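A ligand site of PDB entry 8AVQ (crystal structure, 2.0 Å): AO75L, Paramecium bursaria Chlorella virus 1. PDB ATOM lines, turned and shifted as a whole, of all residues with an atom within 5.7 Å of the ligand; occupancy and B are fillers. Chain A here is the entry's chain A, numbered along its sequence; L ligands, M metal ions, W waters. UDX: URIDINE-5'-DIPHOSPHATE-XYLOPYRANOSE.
The backbone carbonyl oxygen (O) of Lys 178 sits close to an oxygen (O4) of the ligand. Ile 128 touches the ligand. CA of Gly 179 touches O4 of the ligand, at 3.7 Å. Gly 185 touches the ligand (O to N3, 3.8 Å). Phe 189 touches the ligand (CB to N3, 3.4 Å). Gly 204 touches the ligand. Asp 208 touches the ligand (O to C5', 3.4 Å). His 210 touches the ligand. Hydrophobic or aromatic side chains that line the ligand: Ile 128, His 186, Phe 189 and His 210. Within 4 Å of the ligand: Asp 76, Ile 128, Asn 151, Thr 153, Asn 156, Arg 161, Lys 178, Gly 179, Glu 180, Gly 185, His 186, Phe 189, Gly 204, Gly 206, Asp 208, Thr 209, His 210, Arg 211 and Glu 214. The nearest printed residue that does not touch the ligand is Ile 152 (4.002 Å).
An oxygen (O1A) of the ligand is in hydrogen-bond range of the backbone NH of Thr 153 (3.2 Å). OG1 of Thr 153 is in hydrogen-bond range of O2A of the ligand, 2.6 Å away. An oxygen (O3D) of the ligand lies within hydrogen-bond range of the side-chain carboxylate of Glu 214 (2.6 Å). O4' of the ligand lies within hydrogen-bond range of OD1 of Asp 76 (2.7 Å). O1B of the ligand lies within hydrogen-bond range of ND2 of Asn 156. The guanidinium group (NH2) of Arg 211 is in salt-bridge range of an oxygen (O1A) of the ligand (2.9 Å). An oxygen (O1B) of the ligand is in salt-bridge range of the guanidinium group of Arg 161 (2.9 Å). O4' of the ligand lies within hydrogen-bond range of N of Gly 206, at 3.0 Å. An oxygen (O4) of the ligand is in hydrogen-bond range of the backbone NH of Glu 180 (3.2 Å). O of Glu 180 is in hydrogen-bond range of N3 of the ligand. The side-chain amide nitrogen of Asn 151 lies within hydrogen-bond range of an oxygen (O4) of the ligand, 3.1 Å away. The side-chain hydroxyl of Thr 209 lies within hydrogen-bond range of an oxygen (O5') of the ligand, 3.2 Å away. A ring nitrogen (ND1) of His 186 sits at hydrogen-bond distance from an oxygen (O2) of the ligand (3.3 Å).
The backbone NH (N) of Arg 211 sits close to the side-chain carboxylate (OE1) of Glu 214. The guanidinium group (NH1) of Arg 161 lies within hydrogen-bond range of the backbone carbonyl oxygen (O) of Pro 202, 3.1 Å away. O of Arg 203 is in hydrogen-bond range of NE of Arg 161, at 2.9 Å. OG of Ser 182 lies within hydrogen-bond range of OE2 of Glu 180, 3.2 Å away. ND2 of Asn 151 is in hydrogen-bond range of O of Lys 178 (3.4 Å). ND2 of Asn 151 lies within hydrogen-bond range of OH of Tyr 149, at 2.9 Å. The side-chain hydroxyl (OG1) of Thr 115 sits close to a ring nitrogen (NE2) of His 210 (3.3 Å). The side-chain hydroxyl (OG) of Ser 182 sits at hydrogen-bond distance from the backbone NH (N) of Gly 185 (2.9 Å).
Water W3 bridges O2A of the ligand (2.6 Å) and ND2 of Asn 156 (2.6 Å). Water W5 lies within hydrogen-bond range of the side-chain carboxylate of Asp 76 (2.5 Å) and an oxygen (O3') of the ligand (2.7 Å). Water W7 lies within hydrogen-bond range of N of Asn 205 (2.7 Å) and O1B of the ligand (2.8 Å). Water W4 lies within hydrogen-bond range of O3D of the ligand (2.8 Å), N of Arg 211 (2.9 Å) and N of His 210 (3.1 Å). Water W8 lies within hydrogen-bond range of the side-chain amide oxygen (OD1) of Asn 151 (2.8 Å), the guanidinium group (NH2) of Arg 211 (3.3 Å) and the side-chain hydroxyl (OG1) of Thr 153 (3.4 Å). Water W2 bridges O of Asp 208 (2.6 Å) and O4' of the ligand (3.5 Å).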
ATOM      1  N   ASP A  76     -28.422   6.876 -16.863  1.00  0.00           N
ATOM      2  CA  ASP A  76     -29.038   5.562 -16.537  1.00  0.00           C
ATOM      3  C   ASP A  76     -30.546   5.590 -16.832  1.00  0.00           C
ATOM      4  O   ASP A  76     -31.176   4.521 -16.707  1.00  0.00           O
ATOM      5  CB  ASP A  76     -28.831   5.202 -15.067  1.00  0.00           C
ATOM      6  CG  ASP A  76     -27.381   4.928 -14.697  1.00  0.00           C
ATOM      7  OD1 ASP A  76     -26.560   4.776 -15.627  1.00  0.00           O
ATOM      8  OD2 ASP A  76     -27.097   4.851 -13.485  1.00  0.00           O
ATOM      9  N   LEU A 112     -24.664   1.288 -25.375  1.00  0.00           N
ATOM     10  CA  LEU A 112     -23.990   2.117 -24.340  1.00  0.00           C
ATOM     11  C   LEU A 112     -22.498   2.141 -24.671  1.00  0.00           C
ATOM     12  O   LEU A 112     -21.896   3.227 -24.612  1.00  0.00           O
ATOM     13  CB  LEU A 112     -24.246   1.527 -22.951  1.00  0.00           C
ATOM     14  CG  LEU A 112     -23.539   2.221 -21.783  1.00  0.00           C
ATOM     15  CD1 LEU A 112     -23.772   3.719 -21.806  1.00  0.00           C
ATOM     16  CD2 LEU A 112     -23.978   1.640 -20.447  1.00  0.00           C
ATOM     17  N   THR A 115     -17.106   3.122 -21.387  1.00  0.00           N
ATOM     18  CA  THR A 115     -17.002   4.337 -20.540  1.00  0.00           C
ATOM     19  C   THR A 115     -16.272   5.441 -21.320  1.00  0.00           C
ATOM     20  O   THR A 115     -15.281   5.138 -22.011  1.00  0.00           O
ATOM     21  CB  THR A 115     -16.300   4.012 -19.216  1.00  0.00           C
ATOM     22  OG1 THR A 115     -17.125   3.074 -18.521  1.00  0.00           O
ATOM     23  CG2 THR A 115     -16.047   5.221 -18.348  1.00  0.00           C
ATOM     24  N   ILE A 128     -11.281   3.085 -16.649  1.00  0.00           N
ATOM     25  CA  ILE A 128     -12.173   2.046 -17.259  1.00  0.00           C
ATOM     26  C   ILE A 128     -12.633   2.488 -18.652  1.00  0.00           C
ATOM     27  O   ILE A 128     -13.265   1.662 -19.351  1.00  0.00           O
ATOM     28  CB  ILE A 128     -13.340   1.673 -16.324  1.00  0.00           C
ATOM     29  CG1 ILE A 128     -14.358   2.806 -16.168  1.00  0.00           C
ATOM     30  CG2 ILE A 128     -12.824   1.184 -14.984  1.00  0.00           C
ATOM     31  CD1 ILE A 128     -15.646   2.400 -15.486  1.00  0.00           C
ATOM     32  N   TYR A 149     -17.120 -16.166 -16.647  1.00  0.00           N
ATOM     33  CA  TYR A 149     -16.502 -15.169 -15.744  1.00  0.00           C
ATOM     34  C   TYR A 149     -17.581 -14.406 -14.984  1.00  0.00           C
ATOM     35  O   TYR A 149     -18.545 -13.922 -15.586  1.00  0.00           O
ATOM     36  CB  TYR A 149     -15.633 -14.213 -16.550  1.00  0.00           C
ATOM     37  CG  TYR A 149     -14.857 -13.229 -15.716  1.00  0.00           C
ATOM     38  CD1 TYR A 149     -13.944 -13.640 -14.760  1.00  0.00           C
ATOM     39  CD2 TYR A 149     -15.034 -11.861 -15.892  1.00  0.00           C
ATOM     40  CE1 TYR A 149     -13.228 -12.732 -14.004  1.00  0.00           C
ATOM     41  CE2 TYR A 149     -14.320 -10.943 -15.150  1.00  0.00           C
ATOM     42  CZ  TYR A 149     -13.412 -11.370 -14.199  1.00  0.00           C
ATOM     43  OH  TYR A 149     -12.717 -10.453 -13.470  1.00  0.00           O
ATOM     44  N   ASN A 151     -17.911 -11.182 -12.361  1.00  0.00           N
ATOM     45  CA  ASN A 151     -17.285 -10.033 -11.732  1.00  0.00           C
ATOM     46  C   ASN A 151     -18.254  -8.853 -11.884  1.00  0.00           C
ATOM     47  O   ASN A 151     -18.128  -8.099 -12.879  1.00  0.00           O
ATOM     48  CB  ASN A 151     -15.909  -9.712 -12.315  1.00  0.00           C
ATOM     49  CG  ASN A 151     -15.189  -8.621 -11.543  1.00  0.00           C
ATOM     50  OD1 ASN A 151     -15.819  -7.806 -10.871  1.00  0.00           O
ATOM     51  ND2 ASN A 151     -13.872  -8.596 -11.640  1.00  0.00           N
ATOM     52  N   ILE A 152     -19.210  -8.757 -10.954  1.00  0.00           N
ATOM     53  CA  ILE A 152     -20.328  -7.787 -10.982  1.00  0.00           C
ATOM     54  C   ILE A 152     -20.448  -7.136  -9.604  1.00  0.00           C
ATOM     55  O   ILE A 152     -20.172  -7.822  -8.595  1.00  0.00           O
ATOM     56  CB  ILE A 152     -21.635  -8.469 -11.424  1.00  0.00           C
ATOM     57  CG1 ILE A 152     -22.037  -9.603 -10.477  1.00  0.00           C
ATOM     58  CG2 ILE A 152     -21.515  -8.950 -12.857  1.00  0.00           C
ATOM     59  CD1 ILE A 152     -23.344 -10.273 -10.834  1.00  0.00           C
ATOM     60  N   THR A 153     -20.852  -5.875  -9.554  1.00  0.00           N
ATOM     61  CA  THR A 153     -21.222  -5.152  -8.319  1.00  0.00           C
ATOM     62  C   THR A 153     -22.702  -5.446  -8.055  1.00  0.00           C
ATOM     63  O   THR A 153     -23.534  -4.871  -8.787  1.00  0.00           O
ATOM     64  CB  THR A 153     -20.899  -3.663  -8.433  1.00  0.00           C
ATOM     65  OG1 THR A 153     -19.563  -3.551  -8.936  1.00  0.00           O
ATOM     66  CG2 THR A 153     -21.028  -2.932  -7.117  1.00  0.00           C
ATOM     67  N   ASN A 156     -25.778  -2.774  -7.414  1.00  0.00           N
ATOM     68  CA  ASN A 156     -26.281  -1.915  -8.523  1.00  0.00           C
ATOM     69  C   ASN A 156     -27.655  -2.400  -9.057  1.00  0.00           C
ATOM     70  O   ASN A 156     -28.412  -1.534  -9.518  1.00  0.00           O
ATOM     71  CB  ASN A 156     -25.243  -1.798  -9.640  1.00  0.00           C
ATOM     72  CG  ASN A 156     -24.025  -1.008  -9.203  1.00  0.00           C
ATOM     73  OD1 ASN A 156     -24.037  -0.380  -8.159  1.00  0.00           O
ATOM     74  ND2 ASN A 156     -22.960  -1.056 -10.000  1.00  0.00           N
ATOM     75  N   ARG A 161     -28.699  -9.503  -9.809  1.00  0.00           N
ATOM     76  CA  ARG A 161     -27.248  -9.739  -9.559  1.00  0.00           C
ATOM     77  C   ARG A 161     -27.043 -10.619  -8.318  1.00  0.00           C
ATOM     78  O   ARG A 161     -26.076 -11.413  -8.321  1.00  0.00           O
ATOM     79  CB  ARG A 161     -26.504  -8.411  -9.453  1.00  0.00           C
ATOM     80  CG  ARG A 161     -26.543  -7.599 -10.741  1.00  0.00           C
ATOM     81  CD  ARG A 161     -25.471  -6.532 -10.794  1.00  0.00           C
ATOM     82  NE  ARG A 161     -25.416  -5.897 -12.106  1.00  0.00           N
ATOM     83  CZ  ARG A 161     -24.431  -5.105 -12.527  1.00  0.00           C
ATOM     84  NH1 ARG A 161     -24.487  -4.582 -13.745  1.00  0.00           N
ATOM     85  NH2 ARG A 161     -23.390  -4.836 -11.754  1.00  0.00           N
ATOM     86  N   LYS A 178     -12.656 -10.479  -8.213  1.00  0.00           N
ATOM     87  CA  LYS A 178     -12.825  -9.387  -7.217  1.00  0.00           C
ATOM     88  C   LYS A 178     -12.864  -8.045  -7.959  1.00  0.00           C
ATOM     89  O   LYS A 178     -12.056  -7.867  -8.892  1.00  0.00           O
ATOM     90  CB  LYS A 178     -11.680  -9.435  -6.192  1.00  0.00           C
ATOM     91  CG  LYS A 178     -11.788  -8.449  -5.027  1.00  0.00           C
ATOM     92  CD  LYS A 178     -10.439  -8.115  -4.411  1.00  0.00           C
ATOM     93  CE  LYS A 178     -10.537  -7.267  -3.159  1.00  0.00           C
ATOM     94  NZ  LYS A 178     -10.716  -5.827  -3.464  1.00  0.00           N
ATOM     95  N   GLY A 179     -13.788  -7.163  -7.587  1.00  0.00           N
ATOM     96  CA  GLY A 179     -13.898  -5.797  -8.142  1.00  0.00           C
ATOM     97  C   GLY A 179     -12.702  -4.949  -7.767  1.00  0.00           C
ATOM     98  O   GLY A 179     -12.487  -4.735  -6.559  1.00  0.00           O
ATOM     99  N   GLU A 180     -11.930  -4.493  -8.758  1.00  0.00           N
ATOM    100  CA  GLU A 180     -10.776  -3.565  -8.574  1.00  0.00           C
ATOM    101  C   GLU A 180     -10.678  -2.647  -9.800  1.00  0.00           C
ATOM    102  O   GLU A 180     -10.492  -3.170 -10.906  1.00  0.00           O
ATOM    103  CB  GLU A 180      -9.478  -4.340  -8.346  1.00  0.00           C
ATOM    104  CG  GLU A 180      -8.304  -3.434  -8.010  1.00  0.00           C
ATOM    105  CD  GLU A 180      -7.067  -4.119  -7.451  1.00  0.00           C
ATOM    106  OE1 GLU A 180      -7.155  -5.305  -7.076  1.00  0.00           O
ATOM    107  OE2 GLU A 180      -6.009  -3.449  -7.395  1.00  0.00           O
ATOM    108  N   VAL A 181     -10.788  -1.333  -9.591  1.00  0.00           N
ATOM    109  CA  VAL A 181     -10.947  -0.300 -10.658  1.00  0.00           C
ATOM    110  C   VAL A 181      -9.682   0.572 -10.724  1.00  0.00           C
ATOM    111  O   VAL A 181      -9.784   1.737 -11.130  1.00  0.00           O
ATOM    112  CB  VAL A 181     -12.223   0.525 -10.456  1.00  0.00           C
ATOM    113  CG1 VAL A 181     -13.473  -0.312 -10.725  1.00  0.00           C
ATOM    114  CG2 VAL A 181     -12.307   1.164  -9.077  1.00  0.00           C
ATOM    115  N   SER A 182      -8.529   0.012 -10.352  1.00  0.00           N
ATOM    116  CA  SER A 182      -7.172   0.561 -10.645  1.00  0.00           C
ATOM    117  C   SER A 182      -6.824   0.270 -12.106  1.00  0.00           C
ATOM    118  O   SER A 182      -7.548  -0.521 -12.735  1.00  0.00           O
ATOM    119  CB  SER A 182      -6.152  -0.031  -9.717  1.00  0.00           C
ATOM    120  OG  SER A 182      -6.085  -1.435  -9.875  1.00  0.00           O
ATOM    121  N   GLY A 185      -6.105  -3.352 -12.084  1.00  0.00           N
ATOM    122  CA  GLY A 185      -7.393  -4.047 -11.845  1.00  0.00           C
ATOM    123  C   GLY A 185      -8.255  -4.096 -13.099  1.00  0.00           C
ATOM    124  O   GLY A 185      -8.920  -5.128 -13.323  1.00  0.00           O
ATOM    125  N   HIS A 186      -8.250  -3.014 -13.889  1.00  0.00           N
ATOM    126  CA  HIS A 186      -8.985  -2.880 -15.173  1.00  0.00           C
ATOM    127  C   HIS A 186      -8.363  -3.808 -16.232  1.00  0.00           C
ATOM    128  O   HIS A 186      -9.121  -4.465 -16.949  1.00  0.00           O
ATOM    129  CB  HIS A 186      -9.025  -1.430 -15.645  1.00  0.00           C
ATOM    130  CG  HIS A 186      -9.680  -1.230 -16.966  1.00  0.00           C
ATOM    131  ND1 HIS A 186     -10.977  -1.627 -17.210  1.00  0.00           N
ATOM    132  CD2 HIS A 186      -9.232  -0.680 -18.110  1.00  0.00           C
ATOM    133  CE1 HIS A 186     -11.300  -1.322 -18.455  1.00  0.00           C
ATOM    134  NE2 HIS A 186     -10.245  -0.736 -19.027  1.00  0.00           N
ATOM    135  N   PHE A 189      -9.228  -7.361 -15.217  1.00  0.00           N
ATOM    136  CA  PHE A 189     -10.666  -7.552 -15.559  1.00  0.00           C
ATOM    137  C   PHE A 189     -10.796  -7.974 -17.032  1.00  0.00           C
ATOM    138  O   PHE A 189     -11.455  -8.989 -17.297  1.00  0.00           O
ATOM    139  CB  PHE A 189     -11.452  -6.274 -15.267  1.00  0.00           C
ATOM    140  CG  PHE A 189     -12.887  -6.304 -15.740  1.00  0.00           C
ATOM    141  CD1 PHE A 189     -13.847  -7.019 -15.039  1.00  0.00           C
ATOM    142  CD2 PHE A 189     -13.263  -5.624 -16.885  1.00  0.00           C
ATOM    143  CE1 PHE A 189     -15.164  -7.042 -15.483  1.00  0.00           C
ATOM    144  CE2 PHE A 189     -14.584  -5.650 -17.316  1.00  0.00           C
ATOM    145  CZ  PHE A 189     -15.523  -6.363 -16.623  1.00  0.00           C
ATOM    146  N   PRO A 202     -25.429  -9.047 -16.358  1.00  0.00           N
ATOM    147  CA  PRO A 202     -26.750  -8.580 -15.935  1.00  0.00           C
ATOM    148  C   PRO A 202     -26.830  -7.050 -16.003  1.00  0.00           C
ATOM    149  O   PRO A 202     -25.811  -6.406 -15.903  1.00  0.00           O
ATOM    150  CB  PRO A 202     -26.872  -9.067 -14.492  1.00  0.00           C
ATOM    151  CG  PRO A 202     -25.440  -9.159 -14.030  1.00  0.00           C
ATOM    152  CD  PRO A 202     -24.691  -9.661 -15.249  1.00  0.00           C
ATOM    153  N   ARG A 203     -28.039  -6.528 -16.189  1.00  0.00           N
ATOM    154  CA  ARG A 203     -28.364  -5.081 -16.130  1.00  0.00           C
ATOM    155  C   ARG A 203     -27.909  -4.511 -14.777  1.00  0.00           C
ATOM    156  O   ARG A 203     -27.725  -5.296 -13.839  1.00  0.00           O
ATOM    157  CB  ARG A 203     -29.864  -4.854 -16.336  1.00  0.00           C
ATOM    158  CG  ARG A 203     -30.740  -5.394 -15.205  1.00  0.00           C
ATOM    159  CD  ARG A 203     -32.042  -4.623 -15.066  1.00  0.00           C
ATOM    160  NE  ARG A 203     -31.787  -3.241 -14.697  1.00  0.00           N
ATOM    161  CZ  ARG A 203     -32.707  -2.271 -14.681  1.00  0.00           C
ATOM    162  NH1 ARG A 203     -33.960  -2.528 -15.011  1.00  0.00           N
ATOM    163  NH2 ARG A 203     -32.357  -1.043 -14.329  1.00  0.00           N
ATOM    164  N   GLY A 204     -27.714  -3.193 -14.709  1.00  0.00           N
ATOM    165  CA  GLY A 204     -27.328  -2.476 -13.490  1.00  0.00           C
ATOM    166  C   GLY A 204     -28.374  -1.447 -13.108  1.00  0.00           C
ATOM    167  O   GLY A 204     -29.579  -1.770 -13.242  1.00  0.00           O
ATOM    168  N   ASN A 205     -27.962  -0.286 -12.632  1.00  0.00           N
ATOM    169  CA  ASN A 205     -28.898   0.830 -12.327  1.00  0.00           C
ATOM    170  C   ASN A 205     -29.562   1.242 -13.645  1.00  0.00           C
ATOM    171  O   ASN A 205     -30.807   1.387 -13.664  1.00  0.00           O
ATOM    172  CB  ASN A 205     -28.217   2.016 -11.652  1.00  0.00           C
ATOM    173  CG  ASN A 205     -29.222   2.999 -11.110  1.00  0.00           C
ATOM    174  OD1 ASN A 205     -30.107   2.625 -10.339  1.00  0.00           O
ATOM    175  ND2 ASN A 205     -29.139   4.242 -11.543  1.00  0.00           N
ATOM    176  N   GLY A 206     -28.761   1.403 -14.703  1.00  0.00           N
ATOM    177  CA  GLY A 206     -29.228   1.465 -16.094  1.00  0.00           C
ATOM    178  C   GLY A 206     -29.395   0.060 -16.669  1.00  0.00           C
ATOM    179  O   GLY A 206     -28.678  -0.857 -16.223  1.00  0.00           O
ATOM    180  N   ILE A 207     -30.322  -0.107 -17.612  1.00  0.00           N
ATOM    181  CA  ILE A 207     -30.624  -1.422 -18.246  1.00  0.00           C
ATOM    182  C   ILE A 207     -29.387  -1.884 -19.025  1.00  0.00           C
ATOM    183  O   ILE A 207     -28.913  -3.014 -18.793  1.00  0.00           O
ATOM    184  CB  ILE A 207     -31.851  -1.371 -19.174  1.00  0.00           C
ATOM    185  CG1 ILE A 207     -33.123  -0.919 -18.446  1.00  0.00           C
ATOM    186  CG2 ILE A 207     -32.054  -2.727 -19.847  1.00  0.00           C
ATOM    187  CD1 ILE A 207     -34.111  -0.210 -19.339  1.00  0.00           C
ATOM    188  N   ASP A 208     -28.910  -1.037 -19.948  1.00  0.00           N
ATOM    189  CA  ASP A 208     -27.677  -1.285 -20.737  1.00  0.00           C
ATOM    190  C   ASP A 208     -26.479  -1.127 -19.796  1.00  0.00           C
ATOM    191  O   ASP A 208     -26.564  -0.366 -18.814  1.00  0.00           O
ATOM    192  CB  ASP A 208     -27.610  -0.400 -21.986  1.00  0.00           C
ATOM    193  CG  ASP A 208     -26.699  -0.914 -23.099  1.00  0.00           C
ATOM    194  OD1 ASP A 208     -25.967  -1.892 -22.864  1.00  0.00           O
ATOM    195  OD2 ASP A 208     -26.743  -0.335 -24.203  1.00  0.00           O
ATOM    196  N   THR A 209     -25.397  -1.829 -20.099  1.00  0.00           N
ATOM    197  CA  THR A 209     -24.235  -2.046 -19.202  1.00  0.00           C
ATOM    198  C   THR A 209     -22.978  -1.975 -20.083  1.00  0.00           C
ATOM    199  O   THR A 209     -23.074  -2.398 -21.238  1.00  0.00           O
ATOM    200  CB  THR A 209     -24.506  -3.370 -18.466  1.00  0.00           C
ATOM    201  OG1 THR A 209     -24.928  -3.093 -17.128  1.00  0.00           O
ATOM    202  CG2 THR A 209     -23.335  -4.315 -18.454  1.00  0.00           C
ATOM    203  N   HIS A 210     -21.874  -1.419 -19.585  1.00  0.00           N
ATOM    204  CA  HIS A 210     -20.581  -1.360 -20.322  1.00  0.00           C
ATOM    205  C   HIS A 210     -20.052  -2.789 -20.520  1.00  0.00           C
ATOM    206  O   HIS A 210     -19.496  -3.061 -21.614  1.00  0.00           O
ATOM    207  CB  HIS A 210     -19.535  -0.507 -19.592  1.00  0.00           C
ATOM    208  CG  HIS A 210     -19.939   0.923 -19.387  1.00  0.00           C
ATOM    209  ND1 HIS A 210     -20.259   1.761 -20.430  1.00  0.00           N
ATOM    210  CD2 HIS A 210     -20.062   1.645 -18.258  1.00  0.00           C
ATOM    211  CE1 HIS A 210     -20.573   2.949 -19.955  1.00  0.00           C
ATOM    212  NE2 HIS A 210     -20.456   2.903 -18.620  1.00  0.00           N
ATOM    213  N   ARG A 211     -20.222  -3.646 -19.514  1.00  0.00           N
ATOM    214  CA  ARG A 211     -19.724  -5.049 -19.475  1.00  0.00           C
ATOM    215  C   ARG A 211     -20.212  -5.824 -20.707  1.00  0.00           C
ATOM    216  O   ARG A 211     -19.435  -6.648 -21.224  1.00  0.00           O
ATOM    217  CB  ARG A 211     -20.184  -5.717 -18.185  1.00  0.00           C
ATOM    218  CG  ARG A 211     -19.770  -7.177 -18.033  1.00  0.00           C
ATOM    219  CD  ARG A 211     -20.168  -7.731 -16.686  1.00  0.00           C
ATOM    220  NE  ARG A 211     -19.435  -7.128 -15.582  1.00  0.00           N
ATOM    221  CZ  ARG A 211     -19.864  -6.128 -14.804  1.00  0.00           C
ATOM    222  NH1 ARG A 211     -21.050  -5.567 -14.997  1.00  0.00           N
ATOM    223  NH2 ARG A 211     -19.090  -5.690 -13.827  1.00  0.00           N
ATOM    224  N   GLU A 214     -17.912  -4.564 -23.603  1.00  0.00           N
ATOM    225  CA  GLU A 214     -16.550  -5.018 -23.206  1.00  0.00           C
ATOM    226  C   GLU A 214     -16.380  -6.510 -23.547  1.00  0.00           C
ATOM    227  O   GLU A 214     -15.349  -6.859 -24.154  1.00  0.00           O
ATOM    228  CB  GLU A 214     -16.325  -4.762 -21.716  1.00  0.00           C
ATOM    229  CG  GLU A 214     -16.177  -3.284 -21.374  1.00  0.00           C
ATOM    230  CD  GLU A 214     -16.257  -2.920 -19.893  1.00  0.00           C
ATOM    231  OE1 GLU A 214     -16.850  -3.677 -19.113  1.00  0.00           O
ATOM    232  OE2 GLU A 214     -15.730  -1.850 -19.536  1.00  0.00           O
HETATM  233  C1' UDX L   1     -22.414   0.061 -15.467  1.00  0.00           C
HETATM  234  C2' UDX L   1     -22.282   1.577 -15.460  1.00  0.00           C
HETATM  235  O2' UDX L   1     -21.263   1.976 -14.546  1.00  0.00           O
HETATM  236  C3' UDX L   1     -23.620   2.214 -15.074  1.00  0.00           C
HETATM  237  O3' UDX L   1     -23.510   3.631 -15.132  1.00  0.00           O
HETATM  238  C4' UDX L   1     -24.706   1.709 -16.023  1.00  0.00           C
HETATM  239  O4' UDX L   1     -25.983   2.182 -15.585  1.00  0.00           O
HETATM  240  C5' UDX L   1     -24.713   0.193 -16.045  1.00  0.00           C
HETATM  241  O5' UDX L   1     -23.418  -0.328 -16.390  1.00  0.00           O
HETATM  242  PB  UDX L   1     -22.520  -1.795 -13.543  1.00  0.00           P
HETATM  243  O1B UDX L   1     -23.569  -2.052 -12.518  1.00  0.00           O
HETATM  244  O2B UDX L   1     -22.306  -2.807 -14.621  1.00  0.00           O
HETATM  245  O3B UDX L   1     -22.738  -0.345 -14.166  1.00  0.00           O
HETATM  246  O3A UDX L   1     -21.115  -1.581 -12.808  1.00  0.00           O
HETATM  247  PA  UDX L   1     -20.022  -2.605 -12.248  1.00  0.00           P
HETATM  248  O1A UDX L   1     -20.623  -3.969 -12.146  1.00  0.00           O
HETATM  249  O2A UDX L   1     -19.431  -2.014 -11.009  1.00  0.00           O
HETATM  250  O5D UDX L   1     -18.944  -2.582 -13.433  1.00  0.00           O
HETATM  251  C5D UDX L   1     -18.728  -1.344 -14.158  1.00  0.00           C
HETATM  252  C4D UDX L   1     -17.398  -1.380 -14.874  1.00  0.00           C
HETATM  253  O4D UDX L   1     -16.312  -1.504 -13.928  1.00  0.00           O
HETATM  254  C3D UDX L   1     -17.143  -2.570 -15.811  1.00  0.00           C
HETATM  255  O3D UDX L   1     -17.874  -2.470 -17.033  1.00  0.00           O
HETATM  256  C2D UDX L   1     -15.624  -2.432 -16.006  1.00  0.00           C
HETATM  257  O2D UDX L   1     -15.317  -1.458 -16.984  1.00  0.00           O
HETATM  258  C1D UDX L   1     -15.165  -1.956 -14.619  1.00  0.00           C
HETATM  259  N1  UDX L   1     -14.511  -3.013 -13.814  1.00  0.00           N
HETATM  260  C6  UDX L   1     -15.248  -3.952 -13.130  1.00  0.00           C
HETATM  261  C2  UDX L   1     -13.123  -3.013 -13.745  1.00  0.00           C
HETATM  262  O2  UDX L   1     -12.419  -2.206 -14.338  1.00  0.00           O
HETATM  263  N3  UDX L   1     -12.582  -4.014 -12.977  1.00  0.00           N
HETATM  264  C4  UDX L   1     -13.259  -4.985 -12.275  1.00  0.00           C
HETATM  265  O4  UDX L   1     -12.611  -5.804 -11.618  1.00  0.00           O
HETATM  266  C5  UDX L   1     -14.688  -4.916 -12.379  1.00  0.00           C
HETATM  267 MG    MG M   1     -20.373   4.938 -14.336  1.00  0.00          MG
HETATM  268 MG    MG M   2     -19.156   5.254 -16.744  1.00  0.00          MG
HETATM  269  O   HOH W   1     -22.603   4.704 -17.527  1.00  0.00           O
HETATM  270  O   HOH W   2     -27.413   2.140 -18.760  1.00  0.00           O
HETATM  271  O   HOH W   3     -20.589   0.121 -10.033  1.00  0.00           O
HETATM  272  O   HOH W   4     -20.634  -2.424 -16.924  1.00  0.00           O
HETATM  273  O   HOH W   5     -24.687   4.480 -12.833  1.00  0.00           O
HETATM  274  O   HOH W   6     -22.419   6.521 -13.944  1.00  0.00           O
HETATM  275  O   HOH W   7     -25.304   0.081 -12.400  1.00  0.00           O
HETATM  276  O   HOH W   8     -17.605  -5.598 -10.895  1.00  0.00           O
HETATM  277  O   HOH W   9     -10.028  -6.782 -11.560  1.00  0.00           O
HETATM  278  O   HOH W  10     -21.572   1.975 -11.877  1.00  0.00           O
